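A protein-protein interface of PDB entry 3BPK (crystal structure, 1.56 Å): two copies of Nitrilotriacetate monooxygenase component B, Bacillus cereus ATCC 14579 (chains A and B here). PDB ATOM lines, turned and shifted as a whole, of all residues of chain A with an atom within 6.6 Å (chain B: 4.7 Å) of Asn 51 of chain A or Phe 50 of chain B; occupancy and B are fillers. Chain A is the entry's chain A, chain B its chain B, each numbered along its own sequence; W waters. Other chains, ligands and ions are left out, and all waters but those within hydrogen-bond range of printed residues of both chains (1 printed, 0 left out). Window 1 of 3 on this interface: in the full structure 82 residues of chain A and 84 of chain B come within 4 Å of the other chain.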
ATOM      1  N   SER A  24       7.647   8.704  14.718  1.00  0.00           N
ATOM      2  CA  SER A  24       7.682   8.864  16.188  1.00  0.00           C
ATOM      3  C   SER A  24       6.430   9.501  16.762  1.00  0.00           C
ATOM      4  O   SER A  24       5.916   9.054  17.807  1.00  0.00           O
ATOM      5  CB  SER A  24       8.899   9.701  16.618  1.00  0.00           C
ATOM      6  OG  SER A  24      10.140   9.148  16.182  1.00  0.00           O
ATOM      7  N   ILE A  25       5.970  10.570  16.093  1.00  0.00           N
ATOM      8  CA  ILE A  25       4.801  11.351  16.579  1.00  0.00           C
ATOM      9  C   ILE A  25       3.569  10.692  15.963  1.00  0.00           C
ATOM     10  O   ILE A  25       3.088  11.091  14.895  1.00  0.00           O
ATOM     11  CB  ILE A  25       4.968  12.846  16.279  1.00  0.00           C
ATOM     12  CG1 ILE A  25       6.233  13.361  16.988  1.00  0.00           C
ATOM     13  CG2 ILE A  25       3.733  13.630  16.729  1.00  0.00           C
ATOM     14  CD1 ILE A  25       6.625  14.834  16.647  1.00  0.00           C
ATOM     15  N   ILE A  26       3.150   9.616  16.639  1.00  0.00           N
ATOM     16  CA  ILE A  26       2.042   8.777  16.187  1.00  0.00           C
ATOM     17  C   ILE A  26       1.191   8.359  17.361  1.00  0.00           C
ATOM     18  O   ILE A  26       1.669   8.350  18.496  1.00  0.00           O
ATOM     19  CB  ILE A  26       2.529   7.473  15.433  1.00  0.00           C
ATOM     20  CG1 ILE A  26       3.527   6.678  16.277  1.00  0.00           C
ATOM     21  CG2 ILE A  26       3.122   7.848  14.040  1.00  0.00           C
ATOM     22  CD1 ILE A  26       3.612   5.212  15.789  1.00  0.00           C
ATOM     23  N   PRO A  27      -0.090   8.048  17.108  1.00  0.00           N
ATOM     24  CA  PRO A  27      -0.821   8.185  15.834  1.00  0.00           C
ATOM     25  C   PRO A  27      -1.244   9.668  15.672  1.00  0.00           C
ATOM     26  O   PRO A  27      -1.343  10.401  16.669  1.00  0.00           O
ATOM     27  CB  PRO A  27      -2.063   7.315  16.044  1.00  0.00           C
ATOM     28  CG  PRO A  27      -2.334   7.426  17.552  1.00  0.00           C
ATOM     29  CD  PRO A  27      -0.937   7.533  18.202  1.00  0.00           C
ATOM     30  N   ARG A  28      -1.491  10.104  14.442  1.00  0.00           N
ATOM     31  CA  ARG A  28      -1.945  11.485  14.188  1.00  0.00           C
ATOM     32  C   ARG A  28      -3.339  11.510  13.594  1.00  0.00           C
ATOM     33  O   ARG A  28      -3.602  10.852  12.598  1.00  0.00           O
ATOM     34  CB  ARG A  28      -0.988  12.161  13.206  1.00  0.00           C
ATOM     35  CG  ARG A  28       0.430  12.343  13.783  1.00  0.00           C
ATOM     36  CD  ARG A  28       1.340  13.131  12.797  1.00  0.00           C
ATOM     37  NE  ARG A  28       1.421  12.545  11.446  1.00  0.00           N
ATOM     38  CZ  ARG A  28       2.139  11.456  11.137  1.00  0.00           C
ATOM     39  NH1 ARG A  28       2.839  10.801  12.091  1.00  0.00           N
ATOM     40  NH2 ARG A  28       2.179  11.017   9.861  1.00  0.00           N
ATOM     41  N   PRO A  29      -4.215  12.329  14.171  1.00  0.00           N
ATOM     42  CA  PRO A  29      -5.576  12.409  13.609  1.00  0.00           C
ATOM     43  C   PRO A  29      -5.513  13.114  12.258  1.00  0.00           C
ATOM     44  O   PRO A  29      -4.622  13.948  12.040  1.00  0.00           O
ATOM     45  CB  PRO A  29      -6.324  13.242  14.650  1.00  0.00           C
ATOM     46  CG  PRO A  29      -5.229  14.161  15.288  1.00  0.00           C
ATOM     47  CD  PRO A  29      -3.992  13.271  15.302  1.00  0.00           C
ATOM     48  N   SER A  48      -2.484  15.398   8.231  1.00  0.00           N
ATOM     49  CA  SER A  48      -2.378  14.762   9.539  1.00  0.00           C
ATOM     50  C   SER A  48      -1.633  15.605  10.588  1.00  0.00           C
ATOM     51  O   SER A  48      -1.577  15.207  11.746  1.00  0.00           O
ATOM     52  CB  SER A  48      -1.699  13.399   9.435  1.00  0.00           C
ATOM     53  OG  SER A  48      -0.296  13.516   9.245  1.00  0.00           O
ATOM     54  N   TYR A  49      -1.126  16.774  10.187  1.00  0.00           N
ATOM     55  CA  TYR A  49      -0.490  17.682  11.164  1.00  0.00           C
ATOM     56  C   TYR A  49      -1.584  18.571  11.748  1.00  0.00           C
ATOM     57  O   TYR A  49      -1.634  19.770  11.477  1.00  0.00           O
ATOM     58  CB  TYR A  49       0.681  18.498  10.589  1.00  0.00           C
ATOM     59  CG  TYR A  49       1.814  17.718   9.969  1.00  0.00           C
ATOM     60  CD1 TYR A  49       1.863  16.325   9.969  1.00  0.00           C
ATOM     61  CD2 TYR A  49       2.861  18.410   9.360  1.00  0.00           C
ATOM     62  CE1 TYR A  49       2.947  15.659   9.371  1.00  0.00           C
ATOM     63  CE2 TYR A  49       3.947  17.751   8.783  1.00  0.00           C
ATOM     64  CZ  TYR A  49       3.954  16.370   8.759  1.00  0.00           C
ATOM     65  OH  TYR A  49       5.022  15.700   8.184  1.00  0.00           O
ATOM     66  N   PHE A  50      -2.429  17.947  12.574  1.00  0.00           N
ATOM     67  CA  PHE A  50      -3.736  18.485  12.947  1.00  0.00           C
ATOM     68  C   PHE A  50      -3.938  18.265  14.434  1.00  0.00           C
ATOM     69  O   PHE A  50      -3.684  17.164  14.952  1.00  0.00           O
ATOM     70  CB  PHE A  50      -4.761  17.619  12.191  1.00  0.00           C
ATOM     71  CG  PHE A  50      -6.213  17.835  12.590  1.00  0.00           C
ATOM     72  CD1 PHE A  50      -6.743  19.129  12.791  1.00  0.00           C
ATOM     73  CD2 PHE A  50      -7.047  16.724  12.718  1.00  0.00           C
ATOM     74  CE1 PHE A  50      -8.121  19.292  13.099  1.00  0.00           C
ATOM     75  CE2 PHE A  50      -8.400  16.888  13.023  1.00  0.00           C
ATOM     76  CZ  PHE A  50      -8.932  18.165  13.241  1.00  0.00           C
ATOM     77  N   ASN A  51      -4.388  19.286  15.141  1.00  0.00           N
ATOM     78  CA  ASN A  51      -4.782  19.050  16.535  1.00  0.00           C
ATOM     79  C   ASN A  51      -5.628  20.227  17.080  1.00  0.00           C
ATOM     80  O   ASN A  51      -5.904  21.226  16.376  1.00  0.00           O
ATOM     81  CB  ASN A  51      -3.541  18.779  17.443  1.00  0.00           C
ATOM     82  CG  ASN A  51      -3.827  17.740  18.506  1.00  0.00           C
ATOM     83  OD1 ASN A  51      -4.884  17.751  19.131  1.00  0.00           O
ATOM     84  ND2 ASN A  51      -2.885  16.802  18.699  1.00  0.00           N
ATOM     85  N   ILE A  52      -6.024  20.077  18.342  1.00  0.00           N
ATOM     86  CA  ILE A  52      -6.715  21.133  19.068  1.00  0.00           C
ATOM     87  C   ILE A  52      -5.687  22.177  19.482  1.00  0.00           C
ATOM     88  O   ILE A  52      -4.549  21.823  19.772  1.00  0.00           O
ATOM     89  CB  ILE A  52      -7.397  20.565  20.293  1.00  0.00           C
ATOM     90  CG1 ILE A  52      -8.353  19.416  19.898  1.00  0.00           C
ATOM     91  CG2 ILE A  52      -8.162  21.653  21.041  1.00  0.00           C
ATOM     92  CD1 ILE A  52      -8.845  18.564  21.084  1.00  0.00           C
ATOM     93  N   VAL A  53      -6.123  23.439  19.565  1.00  0.00           N
ATOM     94  CA  VAL A  53      -5.318  24.486  20.125  1.00  0.00           C
ATOM     95  C   VAL A  53      -5.869  24.928  21.505  1.00  0.00           C
ATOM     96  O   VAL A  53      -5.140  25.021  22.481  1.00  0.00           O
ATOM     97  CB  VAL A  53      -5.197  25.698  19.170  1.00  0.00           C
ATOM     98  CG1 VAL A  53      -4.583  26.893  19.858  1.00  0.00           C
ATOM     99  CG2 VAL A  53      -4.353  25.319  17.985  1.00  0.00           C
ATOM    100  N   LEU A  59     -10.440  26.514  19.062  1.00  0.00           N
ATOM    101  CA  LEU A  59      -9.405  26.749  18.049  1.00  0.00           C
ATOM    102  C   LEU A  59      -8.737  25.421  17.702  1.00  0.00           C
ATOM    103  O   LEU A  59      -8.487  24.589  18.581  1.00  0.00           O
ATOM    104  CB  LEU A  59      -8.301  27.674  18.604  1.00  0.00           C
ATOM    105  CG  LEU A  59      -8.727  29.120  18.938  1.00  0.00           C
ATOM    106  CD1 LEU A  59      -7.588  29.905  19.541  1.00  0.00           C
ATOM    107  CD2 LEU A  59      -9.260  29.874  17.714  1.00  0.00           C
ATOM    108  N   ILE A  60      -8.432  25.270  16.419  1.00  0.00           N
ATOM    109  CA  ILE A  60      -7.729  24.088  15.907  1.00  0.00           C
ATOM    110  C   ILE A  60      -6.555  24.524  15.038  1.00  0.00           C
ATOM    111  O   ILE A  60      -6.497  25.668  14.580  1.00  0.00           O
ATOM    112  CB  ILE A  60      -8.703  23.163  15.140  1.00  0.00           C
ATOM    113  CG1 ILE A  60      -9.307  23.881  13.913  1.00  0.00           C
ATOM    114  CG2 ILE A  60      -9.789  22.652  16.112  1.00  0.00           C
ATOM    115  CD1 ILE A  60      -8.429  23.895  12.651  1.00  0.00           C
ATOM    116  N   SER A  61      -5.629  23.603  14.798  1.00  0.00           N
ATOM    117  CA  SER A  61      -4.453  23.915  13.950  1.00  0.00           C
ATOM    118  C   SER A  61      -4.305  22.868  12.873  1.00  0.00           C
ATOM    119  O   SER A  61      -4.555  21.673  13.096  1.00  0.00           O
ATOM    120  CB  SER A  61      -3.141  23.973  14.782  1.00  0.00           C
ATOM    121  OG  SER A  61      -2.950  22.772  15.496  1.00  0.00           O
ATOM    122  N   VAL A  62      -3.856  23.314  11.708  1.00  0.00           N
ATOM    123  CA  VAL A  62      -3.481  22.393  10.619  1.00  0.00           C
ATOM    124  C   VAL A  62      -2.220  22.966   9.992  1.00  0.00           C
ATOM    125  O   VAL A  62      -2.215  24.100   9.547  1.00  0.00           O
ATOM    126  CB  VAL A  62      -4.589  22.280   9.523  1.00  0.00           C
ATOM    127  CG1 VAL A  62      -4.111  21.331   8.404  1.00  0.00           C
ATOM    128  CG2 VAL A  62      -5.917  21.820  10.115  1.00  0.00           C
ATOM    129  N   ILE B  25     -11.699  15.163  17.905  1.00  0.00           N
ATOM    130  CA  ILE B  25     -10.346  15.203  17.313  1.00  0.00           C
ATOM    131  C   ILE B  25      -9.533  14.167  18.082  1.00  0.00           C
ATOM    132  O   ILE B  25      -8.880  14.438  19.097  1.00  0.00           O
ATOM    133  CB  ILE B  25      -9.741  16.621  17.317  1.00  0.00           C
ATOM    134  CG1 ILE B  25     -10.640  17.574  16.492  1.00  0.00           C
ATOM    135  CG2 ILE B  25      -8.273  16.589  16.806  1.00  0.00           C
ATOM    136  CD1 ILE B  25     -10.278  19.075  16.673  1.00  0.00           C
ATOM    137  N   ARG B  28      -5.349  11.477  19.896  1.00  0.00           N
ATOM    138  CA  ARG B  28      -4.293  12.517  19.900  1.00  0.00           C
ATOM    139  C   ARG B  28      -2.981  11.964  20.497  1.00  0.00           C
ATOM    140  O   ARG B  28      -3.001  11.341  21.551  1.00  0.00           O
ATOM    141  CB  ARG B  28      -4.704  13.735  20.743  1.00  0.00           C
ATOM    142  CG  ARG B  28      -5.939  14.420  20.137  1.00  0.00           C
ATOM    143  CD  ARG B  28      -6.329  15.674  20.921  1.00  0.00           C
ATOM    144  NE  ARG B  28      -6.616  15.471  22.338  1.00  0.00           N
ATOM    145  CZ  ARG B  28      -7.750  14.903  22.800  1.00  0.00           C
ATOM    146  NH1 ARG B  28      -8.698  14.493  21.959  1.00  0.00           N
ATOM    147  NH2 ARG B  28      -7.958  14.769  24.110  1.00  0.00           N
ATOM    148  N   PRO B  29      -1.857  12.220  19.840  1.00  0.00           N
ATOM    149  CA  PRO B  29      -0.585  11.761  20.411  1.00  0.00           C
ATOM    150  C   PRO B  29      -0.270  12.604  21.641  1.00  0.00           C
ATOM    151  O   PRO B  29      -0.659  13.779  21.700  1.00  0.00           O
ATOM    152  CB  PRO B  29       0.425  12.015  19.289  1.00  0.00           C
ATOM    153  CG  PRO B  29      -0.163  13.139  18.494  1.00  0.00           C
ATOM    154  CD  PRO B  29      -1.683  12.946  18.562  1.00  0.00           C
ATOM    155  N   VAL B  30       0.490  12.039  22.577  1.00  0.00           N
ATOM    156  CA  VAL B  30       0.706  12.724  23.861  1.00  0.00           C
ATOM    157  C   VAL B  30       2.185  13.051  24.044  1.00  0.00           C
ATOM    158  O   VAL B  30       3.032  12.124  24.094  1.00  0.00           O
ATOM    159  CB  VAL B  30       0.195  11.827  25.064  1.00  0.00           C
ATOM    160  CG1 VAL B  30       0.404  12.492  26.423  1.00  0.00           C
ATOM    161  CG2 VAL B  30      -1.315  11.515  24.897  1.00  0.00           C
ATOM    162  N   ALA B  31       2.485  14.347  24.112  1.00  0.00           N
ATOM    163  CA  ALA B  31       3.860  14.798  24.365  1.00  0.00           C
ATOM    164  C   ALA B  31       4.104  14.796  25.869  1.00  0.00           C
ATOM    165  O   ALA B  31       3.365  15.450  26.619  1.00  0.00           O
ATOM    166  CB  ALA B  31       4.088  16.209  23.807  1.00  0.00           C
ATOM    167  N   TYR B  47       0.909  16.521  27.464  1.00  0.00           N
ATOM    168  CA  TYR B  47       0.093  17.433  26.644  1.00  0.00           C
ATOM    169  C   TYR B  47      -0.366  16.703  25.394  1.00  0.00           C
ATOM    170  O   TYR B  47       0.490  16.296  24.591  1.00  0.00           O
ATOM    171  CB  TYR B  47       0.923  18.665  26.213  1.00  0.00           C
ATOM    172  CG  TYR B  47       1.364  19.459  27.417  1.00  0.00           C
ATOM    173  CD1 TYR B  47       0.474  20.348  28.043  1.00  0.00           C
ATOM    174  CD2 TYR B  47       2.617  19.252  28.020  1.00  0.00           C
ATOM    175  CE1 TYR B  47       0.833  21.059  29.185  1.00  0.00           C
ATOM    176  CE2 TYR B  47       2.981  19.959  29.175  1.00  0.00           C
ATOM    177  CZ  TYR B  47       2.096  20.854  29.750  1.00  0.00           C
ATOM    178  OH  TYR B  47       2.446  21.519  30.912  1.00  0.00           O
ATOM    179  N   SER B  48      -1.687  16.538  25.201  1.00  0.00           N
ATOM    180  CA  SER B  48      -2.153  15.859  24.010  1.00  0.00           C
ATOM    181  C   SER B  48      -2.405  16.793  22.819  1.00  0.00           C
ATOM    182  O   SER B  48      -2.740  16.309  21.726  1.00  0.00           O
ATOM    183  CB  SER B  48      -3.404  15.024  24.303  1.00  0.00           C
ATOM    184  OG  SER B  48      -4.554  15.879  24.414  1.00  0.00           O
ATOM    185  N   TYR B  49      -2.246  18.117  23.025  1.00  0.00           N
ATOM    186  CA  TYR B  49      -2.434  19.051  21.896  1.00  0.00           C
ATOM    187  C   TYR B  49      -1.071  19.211  21.233  1.00  0.00           C
ATOM    188  O   TYR B  49      -0.413  20.247  21.319  1.00  0.00           O
ATOM    189  CB  TYR B  49      -3.017  20.406  22.308  1.00  0.00           C
ATOM    190  CG  TYR B  49      -4.373  20.388  22.953  1.00  0.00           C
ATOM    191  CD1 TYR B  49      -5.097  19.204  23.192  1.00  0.00           C
ATOM    192  CD2 TYR B  49      -4.917  21.590  23.391  1.00  0.00           C
ATOM    193  CE1 TYR B  49      -6.328  19.246  23.850  1.00  0.00           C
ATOM    194  CE2 TYR B  49      -6.153  21.634  24.019  1.00  0.00           C
ATOM    195  CZ  TYR B  49      -6.848  20.479  24.232  1.00  0.00           C
ATOM    196  OH  TYR B  49      -8.093  20.505  24.863  1.00  0.00           O
ATOM    197  N   PHE B  50      -0.660  18.131  20.568  1.00  0.00           N
ATOM    198  CA  PHE B  50       0.724  17.914  20.126  1.00  0.00           C
ATOM    199  C   PHE B  50       0.713  17.426  18.669  1.00  0.00           C
ATOM    200  O   PHE B  50      -0.058  16.531  18.292  1.00  0.00           O
ATOM    201  CB  PHE B  50       1.254  16.760  20.993  1.00  0.00           C
ATOM    202  CG  PHE B  50       2.604  16.191  20.599  1.00  0.00           C
ATOM    203  CD1 PHE B  50       3.682  17.009  20.233  1.00  0.00           C
ATOM    204  CD2 PHE B  50       2.799  14.812  20.720  1.00  0.00           C
ATOM    205  CE1 PHE B  50       4.944  16.427  19.960  1.00  0.00           C
ATOM    206  CE2 PHE B  50       4.040  14.242  20.466  1.00  0.00           C
ATOM    207  CZ  PHE B  50       5.102  15.042  20.099  1.00  0.00           C
ATOM    208  N   ASN B  51       1.592  17.993  17.847  1.00  0.00           N
ATOM    209  CA  ASN B  51       1.765  17.395  16.519  1.00  0.00           C
ATOM    210  C   ASN B  51       3.039  17.887  15.862  1.00  0.00           C
ATOM    211  O   ASN B  51       3.795  18.705  16.427  1.00  0.00           O
ATOM    212  CB  ASN B  51       0.540  17.634  15.603  1.00  0.00           C
ATOM    213  CG  ASN B  51       0.218  16.429  14.719  1.00  0.00           C
ATOM    214  OD1 ASN B  51       1.106  15.872  14.091  1.00  0.00           O
ATOM    215  ND2 ASN B  51      -1.055  15.994  14.693  1.00  0.00           N
ATOM    216  N   ILE B  60       7.995  20.977  15.809  1.00  0.00           N
ATOM    217  CA  ILE B  60       6.837  20.346  16.474  1.00  0.00           C
ATOM    218  C   ILE B  60       6.065  21.419  17.231  1.00  0.00           C
ATOM    219  O   ILE B  60       6.586  22.524  17.479  1.00  0.00           O
ATOM    220  CB  ILE B  60       7.241  19.187  17.405  1.00  0.00           C
ATOM    221  CG1 ILE B  60       8.124  19.677  18.551  1.00  0.00           C
ATOM    222  CG2 ILE B  60       8.003  18.113  16.593  1.00  0.00           C
ATOM    223  CD1 ILE B  60       7.390  20.325  19.714  1.00  0.00           C
ATOM    224  N   SER B  61       4.809  21.118  17.550  1.00  0.00           N
ATOM    225  CA  SER B  61       3.987  22.073  18.327  1.00  0.00           C
ATOM    226  C   SER B  61       3.371  21.415  19.540  1.00  0.00           C
ATOM    227  O   SER B  61       2.971  20.242  19.489  1.00  0.00           O
ATOM    228  CB  SER B  61       2.860  22.637  17.456  1.00  0.00           C
ATOM    229  OG  SER B  61       2.067  21.592  16.899  1.00  0.00           O
ATOM    230  N   VAL B  62       3.256  22.193  20.622  1.00  0.00           N
ATOM    231  CA  VAL B  62       2.533  21.716  21.808  1.00  0.00           C
ATOM    232  C   VAL B  62       1.744  22.920  22.314  1.00  0.00           C
ATOM    233  O   VAL B  62       2.327  23.978  22.570  1.00  0.00           O
ATOM    234  CB  VAL B  62       3.501  21.275  22.921  1.00  0.00           C
ATOM    235  CG1 VAL B  62       2.728  20.800  24.145  1.00  0.00           C
ATOM    236  CG2 VAL B  62       4.409  20.158  22.440  1.00  0.00           C
ATOM    237  N   VAL B  86      10.862  16.978  24.476  1.00  0.00           N
ATOM    238  CA  VAL B  86       9.581  16.349  24.155  1.00  0.00           C
ATOM    239  C   VAL B  86       9.808  14.846  24.049  1.00  0.00           C
ATOM    240  O   VAL B  86      10.636  14.404  23.228  1.00  0.00           O
ATOM    241  CB  VAL B  86       9.004  16.888  22.832  1.00  0.00           C
ATOM    242  CG1 VAL B  86       7.713  16.097  22.488  1.00  0.00           C
ATOM    243  CG2 VAL B  86       8.718  18.385  22.963  1.00  0.00           C
ATOM    244  N   ILE B  88       8.143  10.976  23.446  1.00  0.00           N
ATOM    245  CA  ILE B  88       6.991  10.188  22.976  1.00  0.00           C
ATOM    246  C   ILE B  88       6.480   9.342  24.154  1.00  0.00           C
ATOM    247  O   ILE B  88       7.259   8.707  24.891  1.00  0.00           O
ATOM    248  CB  ILE B  88       7.406   9.248  21.823  1.00  0.00           C
ATOM    249  CG1 ILE B  88       7.928  10.079  20.637  1.00  0.00           C
ATOM    250  CG2 ILE B  88       6.248   8.331  21.402  1.00  0.00           C
ATOM    251  CD1 ILE B  88       6.970  11.167  20.160  1.00  0.00           C
ATOM    252  N   MET B 136      13.161  14.050  22.131  1.00  0.00           N
ATOM    253  CA  MET B 136      13.659  15.081  21.232  1.00  0.00           C
ATOM    254  C   MET B 136      14.035  16.301  22.030  1.00  0.00           C
ATOM    255  O   MET B 136      13.194  16.876  22.723  1.00  0.00           O
ATOM    256  CB  MET B 136      12.532  15.470  20.262  1.00  0.00           C
ATOM    257  CG  MET B 136      12.214  14.323  19.254  1.00  0.00           C
ATOM    258  SD  MET B 136      10.539  14.618  18.313  1.00  0.00           S
ATOM    259  CE  MET B 136       9.407  14.005  19.763  1.00  0.00           C
HETATM  260  O   HOH W   1       1.566   9.331  21.156  1.00  0.00           O
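Of the 16 printed residues of chain B, 9 touch a printed residue of chain A.
Hydrophobic or aromatic side chains of chain B within 4 Å of the printed part of chain A: Ile 25, Pro 29, Tyr 49, Phe 50, Ile 60 and Ile 88.
Of the 16 printed residues of chain A, 12 touch a printed residue of chain B.
Hydrophobic or aromatic side chains of chain A within 4 Å of the printed part of chain B: Ile 25, Phe 50, Ile 52 and Ile 60.
Water W1 bridges the backbone carbonyl oxygen of Ile 26 of chain A (2.8 Å) and the backbone NH of Val 30 of chain B (3.2 Å).
Ile 25 of chain A touches Phe 50 of chain B, and with the chains exchanged Phe 50 of chain A touches Ile 25 of chain B.
Ile 25 of chain A touches Ile 60 of chain B, and with the chains exchanged Ile 60 of chain A touches Ile 25 of chain B.
Ser 48 of chain A touches Asn 51 of chain B, and with the chains exchanged Asn 51 of chain A touches Ser 48 of chain B.
Tyr 49 of chain A touches Asn 51 of chain B, and with the chains exchanged Asn 51 of chain A touches Tyr 49 of chain B.
Positions printed for both chains: 25, 28, 29, 48, 49, 50, 51, 60, 61 and 62.
CD1 of Ile 88 of chain B touches O of Ser 24 of chain A (3.3 Å).
CG1 of Ile 25 of chain A touches CD1 of Ile 88 of chain B (3.9 Å).
Pro 29 of chain B touches Ile 26 of chain A.
Pro 27 of chain A touches Pro 29 of chain B (O to CD, 3.2 Å).
CA of Tyr 49 of chain A touches OD1 of Asn 51 of chain B, 3.8 Å away.
Arg 28 of chain B touches Asn 51 of chain A (CD to OD1, 3.1 Å).
CG of Asn 51 of chain A touches CA of Tyr 49 of chain B, 3.9 Å away.
Ile 25 of chain B touches Ile 52 of chain A (CD1 to CG1, 3.8 Å).
Tyr 49 of chain B touches Ile 52 of chain A (CB to O, 3.3 Å).
CD1 of Ile 25 of chain B touches CG2 of Ile 60 of chain A (3.7 Å).
The backbone carbonyl oxygen (O) of Ile 25 of chain B sits at hydrogen-bond distance from the guanidinium group (NH1) of Arg 28 of chain B (2.9 Å).
OG of Ser 48 of chain B is in hydrogen-bond range of NE of Arg 28 of chain B, 3.0 Å away.
The backbone carbonyl oxygen of Leu 59 of chain A is in hydrogen-bond range of the backbone NH of Val 53 of chain A.
The guanidinium group of Arg 28 of chain A lies within hydrogen-bond range of the side-chain hydroxyl of Ser 48 of chain A (3.0 Å).
O of Asn 51 of chain A is in hydrogen-bond range of N of Ser 61 of chain A.
N of Ser 61 of chain B sits at hydrogen-bond distance from O of Asn 51 of chain B (2.8 Å).
O of Ser 48 of chain B is in hydrogen-bond range of ND2 of Asn 51 of chain A.
O of Phe 50 of chain A is in hydrogen-bond range of ND2 of Asn 51 of chain B (2.9 Å).
The side-chain amide nitrogen (ND2) of Asn 51 of chain B lies within hydrogen-bond range of the backbone carbonyl oxygen (O) of Ser 48 of chain A (3.1 Å).
The backbone carbonyl oxygen (O) of Phe 50 of chain B is in hydrogen-bond range of the side-chain amide nitrogen (ND2) of Asn 51 of chain A (2.9 Å).
Asn 51 of chain A touches just these residues of chain B: Arg 28 (3.1 Å), Ser 48 (3.1 Å), Tyr 49 (3.9 Å) and Phe 50 (2.9 Å).
Phe 50 of chain B touches just these residues of chain A: Ile 25 and Asn 51.
Of the printed residues of chain B, Ile 52 of chain A touches Ile 25, Arg 28 and Tyr 49.
Of the printed residues of chain B, Phe 50 of chain A touches Ile 25 and Asn 51.
Printed residues of chain B within 4 Å of Ile 26 of chain A: Pro 29.
Val 62 of chain A touches none of the printed residues of chain B.
Val 86 of chain B touches none of the printed residues of chain A.
The nearest residue of chain B that does not touch Asn 51 of chain A is Pro 29 of chain B (4.04 Å).
The nearest residue of chain A that does not touch Phe 50 of chain B is Phe 50 of chain A (5.0 Å).
The nearest printed residue of chain B that does not touch Ser 48 of chain A is Phe 50 of chain B (6.8 Å).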
